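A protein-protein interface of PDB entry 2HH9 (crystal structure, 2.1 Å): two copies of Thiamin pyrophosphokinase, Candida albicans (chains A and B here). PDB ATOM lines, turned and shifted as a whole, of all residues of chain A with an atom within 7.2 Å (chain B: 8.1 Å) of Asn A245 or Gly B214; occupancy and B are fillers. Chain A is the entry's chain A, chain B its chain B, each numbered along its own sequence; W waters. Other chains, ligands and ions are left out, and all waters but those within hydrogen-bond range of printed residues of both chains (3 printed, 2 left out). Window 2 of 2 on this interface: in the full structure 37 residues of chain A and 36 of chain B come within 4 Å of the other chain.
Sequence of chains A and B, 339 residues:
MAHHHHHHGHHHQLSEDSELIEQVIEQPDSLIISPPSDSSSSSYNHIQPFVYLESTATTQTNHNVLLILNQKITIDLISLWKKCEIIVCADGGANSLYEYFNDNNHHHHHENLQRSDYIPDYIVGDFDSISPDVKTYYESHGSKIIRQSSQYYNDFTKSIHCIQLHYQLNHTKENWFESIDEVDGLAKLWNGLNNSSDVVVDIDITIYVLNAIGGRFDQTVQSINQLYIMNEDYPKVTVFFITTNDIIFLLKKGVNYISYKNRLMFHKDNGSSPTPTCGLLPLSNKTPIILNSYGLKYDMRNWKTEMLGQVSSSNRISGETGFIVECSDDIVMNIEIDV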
ATOM      1  N   ILE A 213      -8.106 -10.374  10.646  1.00  0.00           N
ATOM      2  CA  ILE A 213      -8.093  -9.181  11.481  1.00  0.00           C
ATOM      3  C   ILE A 213      -8.533  -9.502  12.910  1.00  0.00           C
ATOM      4  O   ILE A 213      -9.325 -10.417  13.131  1.00  0.00           O
ATOM      5  CB  ILE A 213      -9.063  -8.116  10.901  1.00  0.00           C
ATOM      6  CG1 ILE A 213      -8.783  -7.907   9.410  1.00  0.00           C
ATOM      7  CG2 ILE A 213      -8.944  -6.814  11.673  1.00  0.00           C
ATOM      8  CD1 ILE A 213      -7.422  -7.301   9.100  1.00  0.00           C
ATOM      9  N   GLY A 214      -8.016  -8.753  13.877  1.00  0.00           N
ATOM     10  CA  GLY A 214      -8.415  -8.970  15.257  1.00  0.00           C
ATOM     11  C   GLY A 214      -7.447  -9.747  16.128  1.00  0.00           C
ATOM     12  O   GLY A 214      -7.457  -9.589  17.348  1.00  0.00           O
ATOM     13  N   GLY A 215      -6.623 -10.590  15.513  1.00  0.00           N
ATOM     14  CA  GLY A 215      -5.661 -11.372  16.271  1.00  0.00           C
ATOM     15  C   GLY A 215      -4.411 -10.573  16.579  1.00  0.00           C
ATOM     16  O   GLY A 215      -4.503  -9.431  17.039  1.00  0.00           O
ATOM     17  N   PHE A 217      -1.694  -8.078  16.255  1.00  0.00           N
ATOM     18  CA  PHE A 217      -1.701  -6.822  15.523  1.00  0.00           C
ATOM     19  C   PHE A 217      -0.796  -6.739  14.291  1.00  0.00           C
ATOM     20  O   PHE A 217      -1.169  -6.124  13.296  1.00  0.00           O
ATOM     21  CB  PHE A 217      -1.378  -5.663  16.477  1.00  0.00           C
ATOM     22  CG  PHE A 217      -1.747  -4.311  15.932  1.00  0.00           C
ATOM     23  CD1 PHE A 217      -3.063  -4.029  15.578  1.00  0.00           C
ATOM     24  CD2 PHE A 217      -0.789  -3.317  15.782  1.00  0.00           C
ATOM     25  CE1 PHE A 217      -3.421  -2.775  15.083  1.00  0.00           C
ATOM     26  CE2 PHE A 217      -1.137  -2.056  15.286  1.00  0.00           C
ATOM     27  CZ  PHE A 217      -2.454  -1.789  14.938  1.00  0.00           C
ATOM     28  N   THR A 220      -2.623  -8.236  11.517  1.00  0.00           N
ATOM     29  CA  THR A 220      -3.708  -7.381  11.062  1.00  0.00           C
ATOM     30  C   THR A 220      -3.123  -6.334  10.122  1.00  0.00           C
ATOM     31  O   THR A 220      -3.649  -6.096   9.038  1.00  0.00           O
ATOM     32  CB  THR A 220      -4.407  -6.672  12.253  1.00  0.00           C
ATOM     33  OG1 THR A 220      -5.199  -7.624  12.971  1.00  0.00           O
ATOM     34  CG2 THR A 220      -5.314  -5.545  11.761  1.00  0.00           C
ATOM     35  N   ILE A 242     -13.924 -10.287   6.320  1.00  0.00           N
ATOM     36  CA  ILE A 242     -15.110 -10.427   7.155  1.00  0.00           C
ATOM     37  C   ILE A 242     -14.635 -10.845   8.535  1.00  0.00           C
ATOM     38  O   ILE A 242     -14.042 -11.910   8.704  1.00  0.00           O
ATOM     39  CB  ILE A 242     -16.089 -11.472   6.591  1.00  0.00           C
ATOM     40  CG1 ILE A 242     -16.582 -11.025   5.208  1.00  0.00           C
ATOM     41  CG2 ILE A 242     -17.274 -11.642   7.539  1.00  0.00           C
ATOM     42  CD1 ILE A 242     -17.524 -12.014   4.542  1.00  0.00           C
ATOM     43  N   THR A 243     -14.872  -9.988   9.519  1.00  0.00           N
ATOM     44  CA  THR A 243     -14.440 -10.270  10.881  1.00  0.00           C
ATOM     45  C   THR A 243     -15.638 -10.448  11.793  1.00  0.00           C
ATOM     46  O   THR A 243     -16.787 -10.435  11.351  1.00  0.00           O
ATOM     47  CB  THR A 243     -13.600  -9.121  11.458  1.00  0.00           C
ATOM     48  OG1 THR A 243     -14.480  -8.078  11.899  1.00  0.00           O
ATOM     49  CG2 THR A 243     -12.656  -8.557  10.398  1.00  0.00           C
ATOM     50  N   THR A 244     -15.351 -10.605  13.077  1.00  0.00           N
ATOM     51  CA  THR A 244     -16.387 -10.782  14.077  1.00  0.00           C
ATOM     52  C   THR A 244     -17.201  -9.496  14.227  1.00  0.00           C
ATOM     53  O   THR A 244     -18.404  -9.539  14.464  1.00  0.00           O
ATOM     54  CB  THR A 244     -15.765 -11.137  15.448  1.00  0.00           C
ATOM     55  OG1 THR A 244     -14.989 -12.337  15.327  1.00  0.00           O
ATOM     56  CG2 THR A 244     -16.856 -11.347  16.491  1.00  0.00           C
ATOM     57  N   ASN A 245     -16.540  -8.357  14.047  1.00  0.00           N
ATOM     58  CA  ASN A 245     -17.190  -7.063  14.219  1.00  0.00           C
ATOM     59  C   ASN A 245     -17.641  -6.307  12.970  1.00  0.00           C
ATOM     60  O   ASN A 245     -18.686  -5.663  12.986  1.00  0.00           O
ATOM     61  CB  ASN A 245     -16.278  -6.176  15.060  1.00  0.00           C
ATOM     62  CG  ASN A 245     -15.900  -6.832  16.372  1.00  0.00           C
ATOM     63  OD1 ASN A 245     -16.750  -7.054  17.231  1.00  0.00           O
ATOM     64  ND2 ASN A 245     -14.625  -7.162  16.525  1.00  0.00           N
ATOM     65  N   ASP A 246     -16.858  -6.356  11.898  1.00  0.00           N
ATOM     66  CA  ASP A 246     -17.236  -5.660  10.673  1.00  0.00           C
ATOM     67  C   ASP A 246     -16.730  -6.343   9.413  1.00  0.00           C
ATOM     68  O   ASP A 246     -16.176  -7.444   9.443  1.00  0.00           O
ATOM     69  CB  ASP A 246     -16.690  -4.213  10.644  1.00  0.00           C
ATOM     70  CG  ASP A 246     -16.125  -3.749  11.973  1.00  0.00           C
ATOM     71  OD1 ASP A 246     -16.901  -3.653  12.948  1.00  0.00           O
ATOM     72  OD2 ASP A 246     -14.905  -3.470  12.040  1.00  0.00           O
ATOM     73  N   ILE A 247     -16.962  -5.661   8.298  1.00  0.00           N
ATOM     74  CA  ILE A 247     -16.484  -6.090   6.999  1.00  0.00           C
ATOM     75  C   ILE A 247     -15.541  -4.951   6.636  1.00  0.00           C
ATOM     76  O   ILE A 247     -15.864  -3.777   6.846  1.00  0.00           O
ATOM     77  CB  ILE A 247     -17.622  -6.215   5.946  1.00  0.00           C
ATOM     78  CG1 ILE A 247     -17.021  -6.617   4.591  1.00  0.00           C
ATOM     79  CG2 ILE A 247     -18.390  -4.900   5.829  1.00  0.00           C
ATOM     80  CD1 ILE A 247     -17.989  -7.318   3.647  1.00  0.00           C
ATOM     81  N   THR A 277     -22.446   1.569  12.214  1.00  0.00           N
ATOM     82  CA  THR A 277     -21.260   2.397  12.323  1.00  0.00           C
ATOM     83  C   THR A 277     -20.272   2.055  11.213  1.00  0.00           C
ATOM     84  O   THR A 277     -20.345   0.984  10.608  1.00  0.00           O
ATOM     85  CB  THR A 277     -20.572   2.202  13.695  1.00  0.00           C
ATOM     86  OG1 THR A 277     -20.203   0.828  13.865  1.00  0.00           O
ATOM     87  CG2 THR A 277     -21.517   2.601  14.811  1.00  0.00           C
ATOM     88  N   ASN A 334     -14.338   0.381   6.868  1.00  0.00           N
ATOM     89  CA  ASN A 334     -14.878  -0.738   7.629  1.00  0.00           C
ATOM     90  C   ASN A 334     -16.337  -0.400   7.919  1.00  0.00           C
ATOM     91  O   ASN A 334     -16.685   0.769   8.097  1.00  0.00           O
ATOM     92  CB  ASN A 334     -14.121  -0.944   8.953  1.00  0.00           C
ATOM     93  CG  ASN A 334     -14.401   0.158   9.979  1.00  0.00           C
ATOM     94  OD1 ASN A 334     -14.096   1.328   9.752  1.00  0.00           O
ATOM     95  ND2 ASN A 334     -14.984  -0.224  11.115  1.00  0.00           N
ATOM     96  N   ILE A 335     -17.186  -1.420   7.929  1.00  0.00           N
ATOM     97  CA  ILE A 335     -18.603  -1.246   8.232  1.00  0.00           C
ATOM     98  C   ILE A 335     -19.029  -2.319   9.222  1.00  0.00           C
ATOM     99  O   ILE A 335     -18.856  -3.519   8.975  1.00  0.00           O
ATOM    100  CB  ILE A 335     -19.499  -1.359   6.978  1.00  0.00           C
ATOM    101  CG1 ILE A 335     -19.143  -0.257   5.973  1.00  0.00           C
ATOM    102  CG2 ILE A 335     -20.963  -1.239   7.391  1.00  0.00           C
ATOM    103  CD1 ILE A 335     -19.872  -0.372   4.625  1.00  0.00           C
ATOM    104  N   GLU A 336     -19.572  -1.876  10.348  1.00  0.00           N
ATOM    105  CA  GLU A 336     -20.037  -2.781  11.389  1.00  0.00           C
ATOM    106  C   GLU A 336     -21.104  -3.724  10.853  1.00  0.00           C
ATOM    107  O   GLU A 336     -21.988  -3.314  10.102  1.00  0.00           O
ATOM    108  CB  GLU A 336     -20.612  -1.979  12.563  1.00  0.00           C
ATOM    109  CG  GLU A 336     -21.447  -2.799  13.541  1.00  0.00           C
ATOM    110  CD  GLU A 336     -22.303  -1.931  14.443  1.00  0.00           C
ATOM    111  OE1 GLU A 336     -22.953  -0.988  13.933  1.00  0.00           O
ATOM    112  OE2 GLU A 336     -22.332  -2.196  15.660  1.00  0.00           O
ATOM    113  N   ILE A 337     -21.006  -4.995  11.228  1.00  0.00           N
ATOM    114  CA  ILE A 337     -21.990  -5.978  10.806  1.00  0.00           C
ATOM    115  C   ILE A 337     -22.669  -6.542  12.045  1.00  0.00           C
ATOM    116  O   ILE A 337     -22.004  -7.013  12.969  1.00  0.00           O
ATOM    117  CB  ILE A 337     -21.352  -7.119   9.992  1.00  0.00           C
ATOM    118  CG1 ILE A 337     -20.875  -6.576   8.640  1.00  0.00           C
ATOM    119  CG2 ILE A 337     -22.368  -8.243   9.784  1.00  0.00           C
ATOM    120  CD1 ILE A 337     -20.395  -7.641   7.670  1.00  0.00           C
ATOM    121  N   ASP A 338     -23.999  -6.465  12.047  1.00  0.00           N
ATOM    122  CA  ASP A 338     -24.845  -6.925  13.145  1.00  0.00           C
ATOM    123  C   ASP A 338     -24.557  -6.191  14.446  1.00  0.00           C
ATOM    124  O   ASP A 338     -25.435  -5.407  14.871  1.00  0.00           O
ATOM    125  CB  ASP A 338     -24.691  -8.432  13.352  1.00  0.00           C
ATOM    126  CG  ASP A 338     -25.304  -9.238  12.224  1.00  0.00           C
ATOM    127  OD1 ASP A 338     -26.531  -9.127  12.013  1.00  0.00           O
ATOM    128  OD2 ASP A 338     -24.561  -9.982  11.546  1.00  0.00           O
ATOM    129  N   GLN B  71     -14.889  -4.119  26.212  1.00  0.00           N
ATOM    130  CA  GLN B  71     -14.665  -5.469  25.692  1.00  0.00           C
ATOM    131  C   GLN B  71     -14.447  -6.380  26.895  1.00  0.00           C
ATOM    132  O   GLN B  71     -14.019  -5.923  27.953  1.00  0.00           O
ATOM    133  CB  GLN B  71     -13.438  -5.531  24.764  1.00  0.00           C
ATOM    134  CG  GLN B  71     -13.631  -4.856  23.406  1.00  0.00           C
ATOM    135  CD  GLN B  71     -12.502  -5.142  22.428  1.00  0.00           C
ATOM    136  OE1 GLN B  71     -12.337  -6.268  21.966  1.00  0.00           O
ATOM    137  NE2 GLN B  71     -11.723  -4.119  22.110  1.00  0.00           N
ATOM    138  N   ASN B 211      -8.813  -3.354  26.079  1.00  0.00           N
ATOM    139  CA  ASN B 211      -9.944  -3.386  25.156  1.00  0.00           C
ATOM    140  C   ASN B 211      -9.996  -2.319  24.055  1.00  0.00           C
ATOM    141  O   ASN B 211     -11.064  -2.055  23.497  1.00  0.00           O
ATOM    142  CB  ASN B 211     -11.246  -3.341  25.971  1.00  0.00           C
ATOM    143  CG  ASN B 211     -11.281  -4.388  27.077  1.00  0.00           C
ATOM    144  OD1 ASN B 211     -10.838  -5.518  26.886  1.00  0.00           O
ATOM    145  ND2 ASN B 211     -11.823  -4.017  28.238  1.00  0.00           N
ATOM    146  N   ALA B 212      -8.855  -1.723  23.727  1.00  0.00           N
ATOM    147  CA  ALA B 212      -8.811  -0.688  22.695  1.00  0.00           C
ATOM    148  C   ALA B 212      -8.487  -1.241  21.311  1.00  0.00           C
ATOM    149  O   ALA B 212      -8.685  -0.560  20.305  1.00  0.00           O
ATOM    150  CB  ALA B 212      -7.784   0.379  23.070  1.00  0.00           C
ATOM    151  N   ILE B 213      -7.994  -2.476  21.267  1.00  0.00           N
ATOM    152  CA  ILE B 213      -7.611  -3.121  20.014  1.00  0.00           C
ATOM    153  C   ILE B 213      -8.338  -4.454  19.803  1.00  0.00           C
ATOM    154  O   ILE B 213      -8.697  -5.133  20.762  1.00  0.00           O
ATOM    155  CB  ILE B 213      -6.083  -3.409  19.999  1.00  0.00           C
ATOM    156  CG1 ILE B 213      -5.297  -2.148  20.375  1.00  0.00           C
ATOM    157  CG2 ILE B 213      -5.659  -3.925  18.628  1.00  0.00           C
ATOM    158  CD1 ILE B 213      -5.371  -1.027  19.350  1.00  0.00           C
ATOM    159  N   GLY B 214      -8.545  -4.828  18.543  1.00  0.00           N
ATOM    160  CA  GLY B 214      -9.191  -6.098  18.250  1.00  0.00           C
ATOM    161  C   GLY B 214     -10.690  -6.053  18.043  1.00  0.00           C
ATOM    162  O   GLY B 214     -11.264  -6.986  17.487  1.00  0.00           O
ATOM    163  N   GLY B 215     -11.329  -4.981  18.500  1.00  0.00           N
ATOM    164  CA  GLY B 215     -12.768  -4.855  18.336  1.00  0.00           C
ATOM    165  C   GLY B 215     -13.106  -4.300  16.966  1.00  0.00           C
ATOM    166  O   GLY B 215     -12.594  -4.785  15.956  1.00  0.00           O
ATOM    167  N   ARG B 216     -13.963  -3.283  16.920  1.00  0.00           N
ATOM    168  CA  ARG B 216     -14.332  -2.683  15.645  1.00  0.00           C
ATOM    169  C   ARG B 216     -13.056  -2.060  15.089  1.00  0.00           C
ATOM    170  O   ARG B 216     -12.346  -1.354  15.803  1.00  0.00           O
ATOM    171  CB  ARG B 216     -15.417  -1.624  15.855  1.00  0.00           C
ATOM    172  CG  ARG B 216     -16.354  -1.445  14.667  1.00  0.00           C
ATOM    173  CD  ARG B 216     -17.474  -0.474  15.014  1.00  0.00           C
ATOM    174  NE  ARG B 216     -16.961   0.864  15.295  1.00  0.00           N
ATOM    175  CZ  ARG B 216     -17.425   1.653  16.257  1.00  0.00           C
ATOM    176  NH1 ARG B 216     -18.409   1.235  17.041  1.00  0.00           N
ATOM    177  NH2 ARG B 216     -16.913   2.866  16.431  1.00  0.00           N
ATOM    178  N   PHE B 217     -12.761  -2.331  13.822  1.00  0.00           N
ATOM    179  CA  PHE B 217     -11.541  -1.837  13.205  1.00  0.00           C
ATOM    180  C   PHE B 217     -11.301  -0.330  13.243  1.00  0.00           C
ATOM    181  O   PHE B 217     -10.165   0.100  13.416  1.00  0.00           O
ATOM    182  CB  PHE B 217     -11.433  -2.332  11.756  1.00  0.00           C
ATOM    183  CG  PHE B 217     -10.043  -2.232  11.196  1.00  0.00           C
ATOM    184  CD1 PHE B 217      -8.976  -2.836  11.851  1.00  0.00           C
ATOM    185  CD2 PHE B 217      -9.794  -1.532  10.023  1.00  0.00           C
ATOM    186  CE1 PHE B 217      -7.678  -2.744  11.349  1.00  0.00           C
ATOM    187  CE2 PHE B 217      -8.498  -1.433   9.511  1.00  0.00           C
ATOM    188  CZ  PHE B 217      -7.442  -2.040  10.175  1.00  0.00           C
ATOM    189  N   ASP B 218     -12.345   0.478  13.078  1.00  0.00           N
ATOM    190  CA  ASP B 218     -12.149   1.928  13.113  1.00  0.00           C
ATOM    191  C   ASP B 218     -11.723   2.395  14.514  1.00  0.00           C
ATOM    192  O   ASP B 218     -11.039   3.407  14.658  1.00  0.00           O
ATOM    193  CB  ASP B 218     -13.424   2.662  12.670  1.00  0.00           C
ATOM    194  CG  ASP B 218     -14.622   2.334  13.538  1.00  0.00           C
ATOM    195  OD1 ASP B 218     -14.973   1.139  13.630  1.00  0.00           O
ATOM    196  OD2 ASP B 218     -15.219   3.272  14.121  1.00  0.00           O
ATOM    197  N   GLN B 219     -12.127   1.656  15.543  1.00  0.00           N
ATOM    198  CA  GLN B 219     -11.753   2.006  16.912  1.00  0.00           C
ATOM    199  C   GLN B 219     -10.280   1.638  17.129  1.00  0.00           C
ATOM    200  O   GLN B 219      -9.552   2.320  17.843  1.00  0.00           O
ATOM    201  CB  GLN B 219     -12.639   1.254  17.912  1.00  0.00           C
ATOM    202  CG  GLN B 219     -14.111   1.656  17.862  1.00  0.00           C
ATOM    203  CD  GLN B 219     -14.986   0.825  18.796  1.00  0.00           C
ATOM    204  OE1 GLN B 219     -15.040  -0.402  18.690  1.00  0.00           O
ATOM    205  NE2 GLN B 219     -15.678   1.492  19.711  1.00  0.00           N
ATOM    206  N   THR B 220      -9.852   0.549  16.500  1.00  0.00           N
ATOM    207  CA  THR B 220      -8.469   0.105  16.601  1.00  0.00           C
ATOM    208  C   THR B 220      -7.565   1.153  15.963  1.00  0.00           C
ATOM    209  O   THR B 220      -6.517   1.512  16.505  1.00  0.00           O
ATOM    210  CB  THR B 220      -8.256  -1.247  15.871  1.00  0.00           C
ATOM    211  OG1 THR B 220      -8.887  -2.292  16.616  1.00  0.00           O
ATOM    212  CG2 THR B 220      -6.771  -1.560  15.734  1.00  0.00           C
ATOM    213  N   VAL B 221      -7.978   1.651  14.807  1.00  0.00           N
ATOM    214  CA  VAL B 221      -7.177   2.639  14.117  1.00  0.00           C
ATOM    215  C   VAL B 221      -7.172   3.987  14.835  1.00  0.00           C
ATOM    216  O   VAL B 221      -6.135   4.639  14.921  1.00  0.00           O
ATOM    217  CB  VAL B 221      -7.653   2.812  12.668  1.00  0.00           C
ATOM    218  CG1 VAL B 221      -6.878   3.942  11.994  1.00  0.00           C
ATOM    219  CG2 VAL B 221      -7.451   1.495  11.906  1.00  0.00           C
ATOM    220  N   SER B 223      -7.387   4.439  17.918  1.00  0.00           N
ATOM    221  CA  SER B 223      -6.515   4.229  19.069  1.00  0.00           C
ATOM    222  C   SER B 223      -5.049   4.380  18.668  1.00  0.00           C
ATOM    223  O   SER B 223      -4.270   5.026  19.360  1.00  0.00           O
ATOM    224  CB  SER B 223      -6.753   2.838  19.661  1.00  0.00           C
ATOM    225  OG  SER B 223      -8.061   2.737  20.198  1.00  0.00           O
ATOM    226  N   THR B 243      -3.574  -6.227  24.964  1.00  0.00           N
ATOM    227  CA  THR B 243      -4.689  -6.932  24.341  1.00  0.00           C
ATOM    228  C   THR B 243      -4.632  -8.415  24.666  1.00  0.00           C
ATOM    229  O   THR B 243      -3.750  -8.876  25.392  1.00  0.00           O
ATOM    230  CB  THR B 243      -4.672  -6.795  22.799  1.00  0.00           C
ATOM    231  OG1 THR B 243      -3.802  -7.793  22.243  1.00  0.00           O
ATOM    232  CG2 THR B 243      -4.165  -5.414  22.389  1.00  0.00           C
ATOM    233  N   THR B 244      -5.582  -9.155  24.110  1.00  0.00           N
ATOM    234  CA  THR B 244      -5.666 -10.589  24.322  1.00  0.00           C
ATOM    235  C   THR B 244      -4.441 -11.288  23.730  1.00  0.00           C
ATOM    236  O   THR B 244      -4.013 -12.334  24.219  1.00  0.00           O
ATOM    237  CB  THR B 244      -6.935 -11.163  23.647  1.00  0.00           C
ATOM    238  OG1 THR B 244      -8.097 -10.490  24.152  1.00  0.00           O
ATOM    239  CG2 THR B 244      -7.060 -12.648  23.921  1.00  0.00           C
ATOM    240  N   ASN B 245      -3.869 -10.688  22.690  1.00  0.00           N
ATOM    241  CA  ASN B 245      -2.730 -11.284  22.008  1.00  0.00           C
ATOM    242  C   ASN B 245      -1.346 -10.670  22.209  1.00  0.00           C
ATOM    243  O   ASN B 245      -0.353 -11.389  22.190  1.00  0.00           O
ATOM    244  CB  ASN B 245      -3.031 -11.351  20.511  1.00  0.00           C
ATOM    245  CG  ASN B 245      -4.403 -11.928  20.222  1.00  0.00           C
ATOM    246  OD1 ASN B 245      -5.422 -11.262  20.401  1.00  0.00           O
ATOM    247  ND2 ASN B 245      -4.434 -13.180  19.785  1.00  0.00           N
ATOM    248  N   ILE B 248       1.133  -3.451  22.731  1.00  0.00           N
ATOM    249  CA  ILE B 248       1.455  -2.551  21.632  1.00  0.00           C
ATOM    250  C   ILE B 248       1.888  -1.199  22.177  1.00  0.00           C
ATOM    251  O   ILE B 248       1.239  -0.635  23.057  1.00  0.00           O
ATOM    252  CB  ILE B 248       0.223  -2.373  20.715  1.00  0.00           C
ATOM    253  CG1 ILE B 248      -0.236  -3.748  20.213  1.00  0.00           C
ATOM    254  CG2 ILE B 248       0.560  -1.441  19.555  1.00  0.00           C
ATOM    255  CD1 ILE B 248      -1.640  -3.760  19.642  1.00  0.00           C
HETATM  256  O   HOH W   1     -12.429  -7.631  15.137  1.00  0.00           O
HETATM  257  O   HOH W   2     -20.022  -1.740  17.278  1.00  0.00           O
HETATM  258  O   HOH W   3      -3.644  -7.295  19.184  1.00  0.00           O
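Ile A213 touches Phe B217, but with the chains exchanged Phe A217 does not touch Ile B213 (4.01 Å). Gly A215 touches Asn B245, and with the chains exchanged Asn A245 touches Gly B215. Phe A217 touches Thr B220, and with the chains exchanged Thr A220 touches Phe B217. Asn A245 touches Gly B214, but with the chains exchanged Gly A214 does not touch Asn B245 (4.03 Å). Of the 13 pairs that touch across the chains among the printed residues, 4 have their exchanged pair printed and touching as well.
Water W1 lies within hydrogen-bond range of ND2 of Asn A245 (2.6 Å), O of Gly B214 (2.7 Å) and O of Gly B215 (3.0 Å). Water W2 lies within hydrogen-bond range of the side-chain carboxylate of Glu A336 (2.9 Å) and the guanidinium group of Arg B216 (3.4 Å). Water W3 lies within hydrogen-bond range of the side-chain hydroxyl of Thr B243 and the backbone carbonyl oxygen of Gly A215.
The side-chain amide nitrogen of Asn A245 is in hydrogen-bond range of the backbone carbonyl oxygen of Gly B215 (3.2 Å). The backbone NH (N) of Phe B217 is in hydrogen-bond range of the side-chain carboxylate (OD2) of Asp A246 (3.0 Å). ND2 of Asn A334 lies within hydrogen-bond range of OD1 of Asp B218.
Along chain A the printed residues that touch a printed residue of chain B span positions 213 to 334. Hydrophobic or aromatic side chains of chain B that line the printed part of chain A: Phe B217 and Ile B248. Along chain B the printed residues that touch a printed residue of chain A span positions 214 to 248.
The backbone NH (N) of Glu A336 sits at hydrogen-bond distance from the backbone carbonyl oxygen (O) of Thr A277, 3.0 Å away. O of Asn A245 sits at hydrogen-bond distance from N of Ile A337, at 3.0 Å. NE of Arg B216 lies within salt-bridge range of OD1 of Asp B218 (2.6 Å). OG1 of Thr A220 lies within hydrogen-bond range of N of Gly A214, 3.2 Å away. The backbone NH (N) of Asn A245 sits at hydrogen-bond distance from the side-chain hydroxyl (OG1) of Thr A243. The side-chain carboxylate of Asp A246 sits at hydrogen-bond distance from the side-chain amide nitrogen of Asn A334 (3.4 Å).
Printed residues of chain B within 4 Å of Ile A213: Phe B217. Asp A246 touches just these residues of chain B: Arg B216 and Phe B217. Of the printed residues of chain B, Thr A277 touches Arg B216. Of the printed residues of chain A, Gly B214 touches Asn A245 (3.5 Å). Of the printed residues of chain A, Asp B218 touches Asn A334. Gln B219 touches none of the printed residues of chain A. The nearest printed residue of chain A that does not touch Gly B214 is Gly A214 (4.001 Å). The nearest printed residue of chain A that does not touch Asp B218 is Asp A246 (4.8 Å).
Among the printed residues, pairs that only touch across the chains: Ile A213 with Phe B217 (3.98 Å), Gly A215 with Asn B245 (3.9 Å), Phe A217 with Thr B220 (3.6 Å), Phe A217 with Ile B248 (3.7 Å), Thr A220 with Phe B217 (3.7 Å), Asn A245 with Gly B214 (3.5 Å), Asn A245 with Arg B216 (3.95 Å), Asp A246 with Arg B216 (2.9 Å), Thr A277 with Arg B216 (3.2 Å) and Asn A334 with Arg B216 (3.998 Å).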
